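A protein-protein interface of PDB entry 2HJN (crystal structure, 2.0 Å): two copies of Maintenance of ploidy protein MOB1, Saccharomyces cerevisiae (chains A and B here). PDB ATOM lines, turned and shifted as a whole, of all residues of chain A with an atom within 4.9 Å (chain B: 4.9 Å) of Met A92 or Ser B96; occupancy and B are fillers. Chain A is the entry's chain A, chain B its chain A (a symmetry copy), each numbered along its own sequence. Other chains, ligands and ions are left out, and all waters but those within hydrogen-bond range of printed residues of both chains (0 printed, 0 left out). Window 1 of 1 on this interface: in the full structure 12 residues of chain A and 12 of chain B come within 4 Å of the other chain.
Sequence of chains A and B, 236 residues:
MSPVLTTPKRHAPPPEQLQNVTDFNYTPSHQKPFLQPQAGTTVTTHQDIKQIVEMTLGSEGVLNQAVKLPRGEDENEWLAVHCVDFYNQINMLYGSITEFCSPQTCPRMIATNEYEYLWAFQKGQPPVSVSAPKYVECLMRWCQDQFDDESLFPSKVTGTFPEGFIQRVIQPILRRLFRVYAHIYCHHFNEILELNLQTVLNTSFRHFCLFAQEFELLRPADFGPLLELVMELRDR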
ATOM      1  N   ASN A  88     -18.425 -18.390  -9.433  1.00  0.00           N
ATOM      2  CA  ASN A  88     -18.977 -18.815 -10.717  1.00  0.00           C
ATOM      3  C   ASN A  88     -18.654 -20.292 -11.069  1.00  0.00           C
ATOM      4  O   ASN A  88     -19.494 -20.991 -11.641  1.00  0.00           O
ATOM      5  CB  ASN A  88     -18.544 -17.831 -11.877  1.00  0.00           C
ATOM      6  CG  ASN A  88     -19.416 -16.567 -11.996  1.00  0.00           C
ATOM      7  OD1 ASN A  88     -20.570 -16.533 -11.601  1.00  0.00           O
ATOM      8  ND2 ASN A  88     -18.852 -15.524 -12.642  1.00  0.00           N
ATOM      9  N   GLN A  89     -17.454 -20.772 -10.727  1.00  0.00           N
ATOM     10  CA  GLN A  89     -17.123 -22.207 -10.883  1.00  0.00           C
ATOM     11  C   GLN A  89     -18.029 -23.094  -9.999  1.00  0.00           C
ATOM     12  O   GLN A  89     -18.496 -24.182 -10.429  1.00  0.00           O
ATOM     13  CB  GLN A  89     -15.608 -22.440 -10.583  1.00  0.00           C
ATOM     14  CG  GLN A  89     -14.688 -21.701 -11.615  1.00  0.00           C
ATOM     15  CD  GLN A  89     -13.224 -21.767 -11.279  1.00  0.00           C
ATOM     16  OE1 GLN A  89     -12.781 -22.713 -10.625  1.00  0.00           O
ATOM     17  NE2 GLN A  89     -12.439 -20.753 -11.731  1.00  0.00           N
ATOM     18  N   ILE A  90     -18.324 -22.639  -8.775  1.00  0.00           N
ATOM     19  CA  ILE A  90     -19.145 -23.457  -7.805  1.00  0.00           C
ATOM     20  C   ILE A  90     -20.618 -23.451  -8.268  1.00  0.00           C
ATOM     21  O   ILE A  90     -21.283 -24.475  -8.282  1.00  0.00           O
ATOM     22  CB  ILE A  90     -19.002 -22.923  -6.366  1.00  0.00           C
ATOM     23  CG1 ILE A  90     -17.628 -23.245  -5.797  1.00  0.00           C
ATOM     24  CG2 ILE A  90     -20.064 -23.530  -5.450  1.00  0.00           C
ATOM     25  CD1 ILE A  90     -17.258 -22.318  -4.539  1.00  0.00           C
ATOM     26  N   ASN A  91     -21.083 -22.290  -8.721  1.00  0.00           N
ATOM     27  CA  ASN A  91     -22.370 -22.164  -9.399  1.00  0.00           C
ATOM     28  C   ASN A  91     -22.531 -23.130 -10.596  1.00  0.00           C
ATOM     29  O   ASN A  91     -23.572 -23.817 -10.699  1.00  0.00           O
ATOM     30  CB  ASN A  91     -22.610 -20.699  -9.880  1.00  0.00           C
ATOM     31  CG  ASN A  91     -23.998 -20.510 -10.427  1.00  0.00           C
ATOM     32  OD1 ASN A  91     -24.999 -20.656  -9.687  1.00  0.00           O
ATOM     33  ND2 ASN A  91     -24.099 -20.204 -11.730  1.00  0.00           N
ATOM     34  N   MET A  92     -21.516 -23.201 -11.470  1.00  0.00           N
ATOM     35  CA  MET A  92     -21.559 -24.116 -12.626  1.00  0.00           C
ATOM     36  C   MET A  92     -21.544 -25.581 -12.174  1.00  0.00           C
ATOM     37  O   MET A  92     -22.328 -26.411 -12.682  1.00  0.00           O
ATOM     38  CB  MET A  92     -20.417 -23.802 -13.629  1.00  0.00           C
ATOM     39  CG  MET A  92     -20.312 -24.838 -14.818  1.00  0.00           C
ATOM     40  SD  MET A  92     -19.334 -26.462 -14.303  1.00  0.00           S
ATOM     41  CE  MET A  92     -17.620 -25.551 -14.125  1.00  0.00           C
ATOM     42  N   LEU A  93     -20.723 -25.891 -11.176  1.00  0.00           N
ATOM     43  CA  LEU A  93     -20.628 -27.265 -10.653  1.00  0.00           C
ATOM     44  C   LEU A  93     -21.895 -27.713  -9.884  1.00  0.00           C
ATOM     45  O   LEU A  93     -22.391 -28.810 -10.100  1.00  0.00           O
ATOM     46  CB  LEU A  93     -19.360 -27.430  -9.821  1.00  0.00           C
ATOM     47  CG  LEU A  93     -18.018 -27.434 -10.602  1.00  0.00           C
ATOM     48  CD1 LEU A  93     -16.896 -27.132  -9.623  1.00  0.00           C
ATOM     49  CD2 LEU A  93     -17.725 -28.754 -11.358  1.00  0.00           C
ATOM     50  N   TYR A  94     -22.463 -26.855  -9.031  1.00  0.00           N
ATOM     51  CA  TYR A  94     -23.760 -27.218  -8.360  1.00  0.00           C
ATOM     52  C   TYR A  94     -24.887 -27.324  -9.335  1.00  0.00           C
ATOM     53  O   TYR A  94     -25.738 -28.223  -9.260  1.00  0.00           O
ATOM     54  CB  TYR A  94     -24.099 -26.276  -7.183  1.00  0.00           C
ATOM     55  CG  TYR A  94     -24.609 -27.016  -5.977  1.00  0.00           C
ATOM     56  CD1 TYR A  94     -23.758 -27.338  -4.928  1.00  0.00           C
ATOM     57  CD2 TYR A  94     -25.934 -27.429  -5.890  1.00  0.00           C
ATOM     58  CE1 TYR A  94     -24.212 -28.052  -3.826  1.00  0.00           C
ATOM     59  CE2 TYR A  94     -26.422 -28.147  -4.752  1.00  0.00           C
ATOM     60  CZ  TYR A  94     -25.548 -28.448  -3.739  1.00  0.00           C
ATOM     61  OH  TYR A  94     -25.982 -29.124  -2.635  1.00  0.00           O
ATOM     62  N   GLY A  95     -24.868 -26.458 -10.305  1.00  0.00           N
ATOM     63  CA  GLY A  95     -25.868 -26.449 -11.347  1.00  0.00           C
ATOM     64  C   GLY A  95     -25.889 -27.726 -12.135  1.00  0.00           C
ATOM     65  O   GLY A  95     -26.930 -28.121 -12.608  1.00  0.00           O
ATOM     66  N   SER A  96     -24.736 -28.355 -12.337  1.00  0.00           N
ATOM     67  CA  SER A  96     -24.684 -29.600 -13.104  1.00  0.00           C
ATOM     68  C   SER A  96     -25.397 -30.780 -12.408  1.00  0.00           C
ATOM     69  O   SER A  96     -25.941 -31.695 -13.063  1.00  0.00           O
ATOM     70  CB  SER A  96     -23.223 -29.969 -13.453  1.00  0.00           C
ATOM     71  OG  SER A  96     -22.556 -30.549 -12.345  1.00  0.00           O
ATOM     72  N   VAL A 200     -12.687 -31.197 -14.013  1.00  0.00           N
ATOM     73  CA  VAL A 200     -13.113 -29.825 -13.809  1.00  0.00           C
ATOM     74  C   VAL A 200     -13.334 -29.560 -12.297  1.00  0.00           C
ATOM     75  O   VAL A 200     -12.948 -28.488 -11.788  1.00  0.00           O
ATOM     76  CB  VAL A 200     -14.382 -29.476 -14.632  1.00  0.00           C
ATOM     77  CG1 VAL A 200     -14.885 -28.073 -14.281  1.00  0.00           C
ATOM     78  CG2 VAL A 200     -14.087 -29.523 -16.089  1.00  0.00           C
ATOM     79  N   MET B  92     -25.922 -30.835 -19.795  1.00  0.00           N
ATOM     80  CA  MET B  92     -25.001 -30.246 -18.805  1.00  0.00           C
ATOM     81  C   MET B  92     -24.212 -29.078 -19.410  1.00  0.00           C
ATOM     82  O   MET B  92     -24.077 -28.008 -18.778  1.00  0.00           O
ATOM     83  CB  MET B  92     -24.069 -31.327 -18.196  1.00  0.00           C
ATOM     84  CG  MET B  92     -22.957 -30.742 -17.238  1.00  0.00           C
ATOM     85  SD  MET B  92     -21.409 -30.052 -18.233  1.00  0.00           S
ATOM     86  CE  MET B  92     -20.833 -31.811 -18.846  1.00  0.00           C
ATOM     87  N   LEU B  93     -23.761 -29.239 -20.650  1.00  0.00           N
ATOM     88  CA  LEU B  93     -22.997 -28.182 -21.336  1.00  0.00           C
ATOM     89  C   LEU B  93     -23.857 -26.948 -21.700  1.00  0.00           C
ATOM     90  O   LEU B  93     -23.444 -25.819 -21.468  1.00  0.00           O
ATOM     91  CB  LEU B  93     -22.269 -28.756 -22.546  1.00  0.00           C
ATOM     92  CG  LEU B  93     -21.067 -29.694 -22.249  1.00  0.00           C
ATOM     93  CD1 LEU B  93     -20.783 -30.515 -23.495  1.00  0.00           C
ATOM     94  CD2 LEU B  93     -19.783 -28.957 -21.792  1.00  0.00           C
ATOM     95  N   TYR B  94     -25.075 -27.145 -22.214  1.00  0.00           N
ATOM     96  CA  TYR B  94     -25.978 -25.968 -22.468  1.00  0.00           C
ATOM     97  C   TYR B  94     -26.389 -25.293 -21.201  1.00  0.00           C
ATOM     98  O   TYR B  94     -26.447 -24.058 -21.102  1.00  0.00           O
ATOM     99  CB  TYR B  94     -27.192 -26.335 -23.350  1.00  0.00           C
ATOM    100  CG  TYR B  94     -27.475 -25.301 -24.404  1.00  0.00           C
ATOM    101  CD1 TYR B  94     -27.012 -25.466 -25.703  1.00  0.00           C
ATOM    102  CD2 TYR B  94     -28.177 -24.139 -24.107  1.00  0.00           C
ATOM    103  CE1 TYR B  94     -27.239 -24.500 -26.676  1.00  0.00           C
ATOM    104  CE2 TYR B  94     -28.437 -23.144 -25.102  1.00  0.00           C
ATOM    105  CZ  TYR B  94     -27.959 -23.343 -26.372  1.00  0.00           C
ATOM    106  OH  TYR B  94     -28.196 -22.418 -27.349  1.00  0.00           O
ATOM    107  N   GLY B  95     -26.608 -26.085 -20.192  1.00  0.00           N
ATOM    108  CA  GLY B  95     -26.981 -25.586 -18.889  1.00  0.00           C
ATOM    109  C   GLY B  95     -25.935 -24.688 -18.296  1.00  0.00           C
ATOM    110  O   GLY B  95     -26.267 -23.785 -17.562  1.00  0.00           O
ATOM    111  N   SER B  96     -24.660 -24.957 -18.555  1.00  0.00           N
ATOM    112  CA  SER B  96     -23.589 -24.128 -18.001  1.00  0.00           C
ATOM    113  C   SER B  96     -23.573 -22.690 -18.565  1.00  0.00           C
ATOM    114  O   SER B  96     -23.167 -21.724 -17.884  1.00  0.00           O
ATOM    115  CB  SER B  96     -22.214 -24.808 -18.191  1.00  0.00           C
ATOM    116  OG  SER B  96     -21.736 -24.652 -19.517  1.00  0.00           O
ATOM    117  N   ILE B  97     -24.038 -22.541 -19.800  1.00  0.00           N
ATOM    118  CA  ILE B  97     -23.985 -21.231 -20.461  1.00  0.00           C
ATOM    119  C   ILE B  97     -25.362 -20.625 -20.773  1.00  0.00           C
ATOM    120  O   ILE B  97     -25.448 -19.603 -21.476  1.00  0.00           O
ATOM    121  CB  ILE B  97     -23.044 -21.237 -21.708  1.00  0.00           C
ATOM    122  CG1 ILE B  97     -23.359 -22.404 -22.668  1.00  0.00           C
ATOM    123  CG2 ILE B  97     -21.615 -21.337 -21.249  1.00  0.00           C
ATOM    124  CD1 ILE B  97     -24.420 -22.120 -23.697  1.00  0.00           C
ATOM    125  N   THR B  98     -26.416 -21.256 -20.251  1.00  0.00           N
ATOM    126  CA  THR B  98     -27.788 -20.929 -20.685  1.00  0.00           C
ATOM    127  C   THR B  98     -28.200 -19.444 -20.508  1.00  0.00           C
ATOM    128  O   THR B  98     -29.013 -18.886 -21.319  1.00  0.00           O
ATOM    129  CB  THR B  98     -28.833 -21.824 -19.965  1.00  0.00           C
ATOM    130  OG1 THR B  98     -30.114 -21.551 -20.520  1.00  0.00           O
ATOM    131  CG2 THR B  98     -28.898 -21.522 -18.430  1.00  0.00           C
ATOM    132  N   PHE B 100     -26.420 -16.962 -21.122  1.00  0.00           N
ATOM    133  CA  PHE B 100     -25.773 -16.176 -22.210  1.00  0.00           C
ATOM    134  C   PHE B 100     -26.429 -16.374 -23.588  1.00  0.00           C
ATOM    135  O   PHE B 100     -26.027 -15.759 -24.566  1.00  0.00           O
ATOM    136  CB  PHE B 100     -24.291 -16.554 -22.307  1.00  0.00           C
ATOM    137  CG  PHE B 100     -23.549 -16.464 -20.977  1.00  0.00           C
ATOM    138  CD1 PHE B 100     -23.053 -17.612 -20.363  1.00  0.00           C
ATOM    139  CD2 PHE B 100     -23.411 -15.250 -20.327  1.00  0.00           C
ATOM    140  CE1 PHE B 100     -22.392 -17.549 -19.131  1.00  0.00           C
ATOM    141  CE2 PHE B 100     -22.749 -15.171 -19.087  1.00  0.00           C
ATOM    142  CZ  PHE B 100     -22.235 -16.330 -18.493  1.00  0.00           C
ATOM    143  N   ILE B 192     -17.704 -20.838 -22.416  1.00  0.00           N
ATOM    144  CA  ILE B 192     -17.284 -22.171 -22.050  1.00  0.00           C
ATOM    145  C   ILE B 192     -15.838 -22.070 -21.475  1.00  0.00           C
ATOM    146  O   ILE B 192     -15.510 -22.634 -20.424  1.00  0.00           O
ATOM    147  CB  ILE B 192     -17.401 -23.121 -23.304  1.00  0.00           C
ATOM    148  CG1 ILE B 192     -18.884 -23.546 -23.589  1.00  0.00           C
ATOM    149  CG2 ILE B 192     -16.392 -24.356 -23.240  1.00  0.00           C
ATOM    150  CD1 ILE B 192     -19.515 -24.278 -22.366  1.00  0.00           C
ATOM    151  N   LEU B 195     -15.426 -20.561 -18.001  1.00  0.00           N
ATOM    152  CA  LEU B 195     -15.786 -21.533 -16.965  1.00  0.00           C
ATOM    153  C   LEU B 195     -14.840 -22.748 -16.952  1.00  0.00           C
ATOM    154  O   LEU B 195     -15.043 -23.715 -16.200  1.00  0.00           O
ATOM    155  CB  LEU B 195     -17.238 -21.967 -17.169  1.00  0.00           C
ATOM    156  CG  LEU B 195     -18.343 -20.906 -16.991  1.00  0.00           C
ATOM    157  CD1 LEU B 195     -19.693 -21.431 -17.475  1.00  0.00           C
ATOM    158  CD2 LEU B 195     -18.389 -20.442 -15.510  1.00  0.00           C
ATOM    159  N   LEU B 197     -14.360 -25.051 -19.241  1.00  0.00           N
ATOM    160  CA  LEU B 197     -15.052 -26.274 -19.684  1.00  0.00           C
ATOM    161  C   LEU B 197     -14.643 -26.698 -21.077  1.00  0.00           C
ATOM    162  O   LEU B 197     -15.286 -27.561 -21.670  1.00  0.00           O
ATOM    163  CB  LEU B 197     -16.565 -26.054 -19.676  1.00  0.00           C
ATOM    164  CG  LEU B 197     -17.185 -26.044 -18.291  1.00  0.00           C
ATOM    165  CD1 LEU B 197     -18.649 -25.472 -18.320  1.00  0.00           C
ATOM    166  CD2 LEU B 197     -17.187 -27.486 -17.808  1.00  0.00           C
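Among the printed residues, pairs that only touch across the chains: Met A92 with Ser B96 (3.9 Å), Met A92 with Leu B195 (3.8 Å), Met A92 with Leu B197 (3.9 Å) and Ser A96 with Met B92 (3.9 Å).
Met A92 touches just these residues of chain B: Ser B96, Leu B195 and Leu B197.
Printed residues of chain A within 4 Å of Leu B197: Met A92 (3.9 Å).
Of the printed residues of chain A, Leu B195 touches Met A92.
Printed residues of chain B within 4 Å of Ser A96: Met B92 (3.9 Å).
Of the printed residues of chain A, Met B92 touches Ser A96 (3.9 Å).
Tyr B94 touches none of the printed residues of chain A.
Val A200 touches none of the printed residues of chain B.
The nearest printed residue of chain A that does not touch Ser B96 is Asn A91 (6.4 Å).
The backbone carbonyl oxygen (O) of Ile B192 is in hydrogen-bond range of the backbone NH (N) of Leu B197.
The backbone carbonyl oxygen (O) of Leu A93 lies within hydrogen-bond range of the side-chain hydroxyl (OG) of Ser A96 (2.8 Å).
The backbone carbonyl oxygen (O) of Leu B93 is in hydrogen-bond range of the side-chain hydroxyl (OG) of Ser B96, at 2.8 Å.
Hydrophobic or aromatic side chains of chain A that line the printed part of chain B: Met A92.
Hydrophobic or aromatic side chains of chain B that line the printed part of chain A: Met B92 and Leu B197.
Among the printed residues, 4 pairs touch across the chains.
Among the printed residues, no Asp or Glu carboxylate lies within 4 Å of a Lys or Arg side-chain nitrogen of the other chain.
Met A92 touches Ser B96, and with the chains exchanged Ser A96 touches Met B92.
Positions printed for both chains: 92, 93, 94, 95 and 96.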
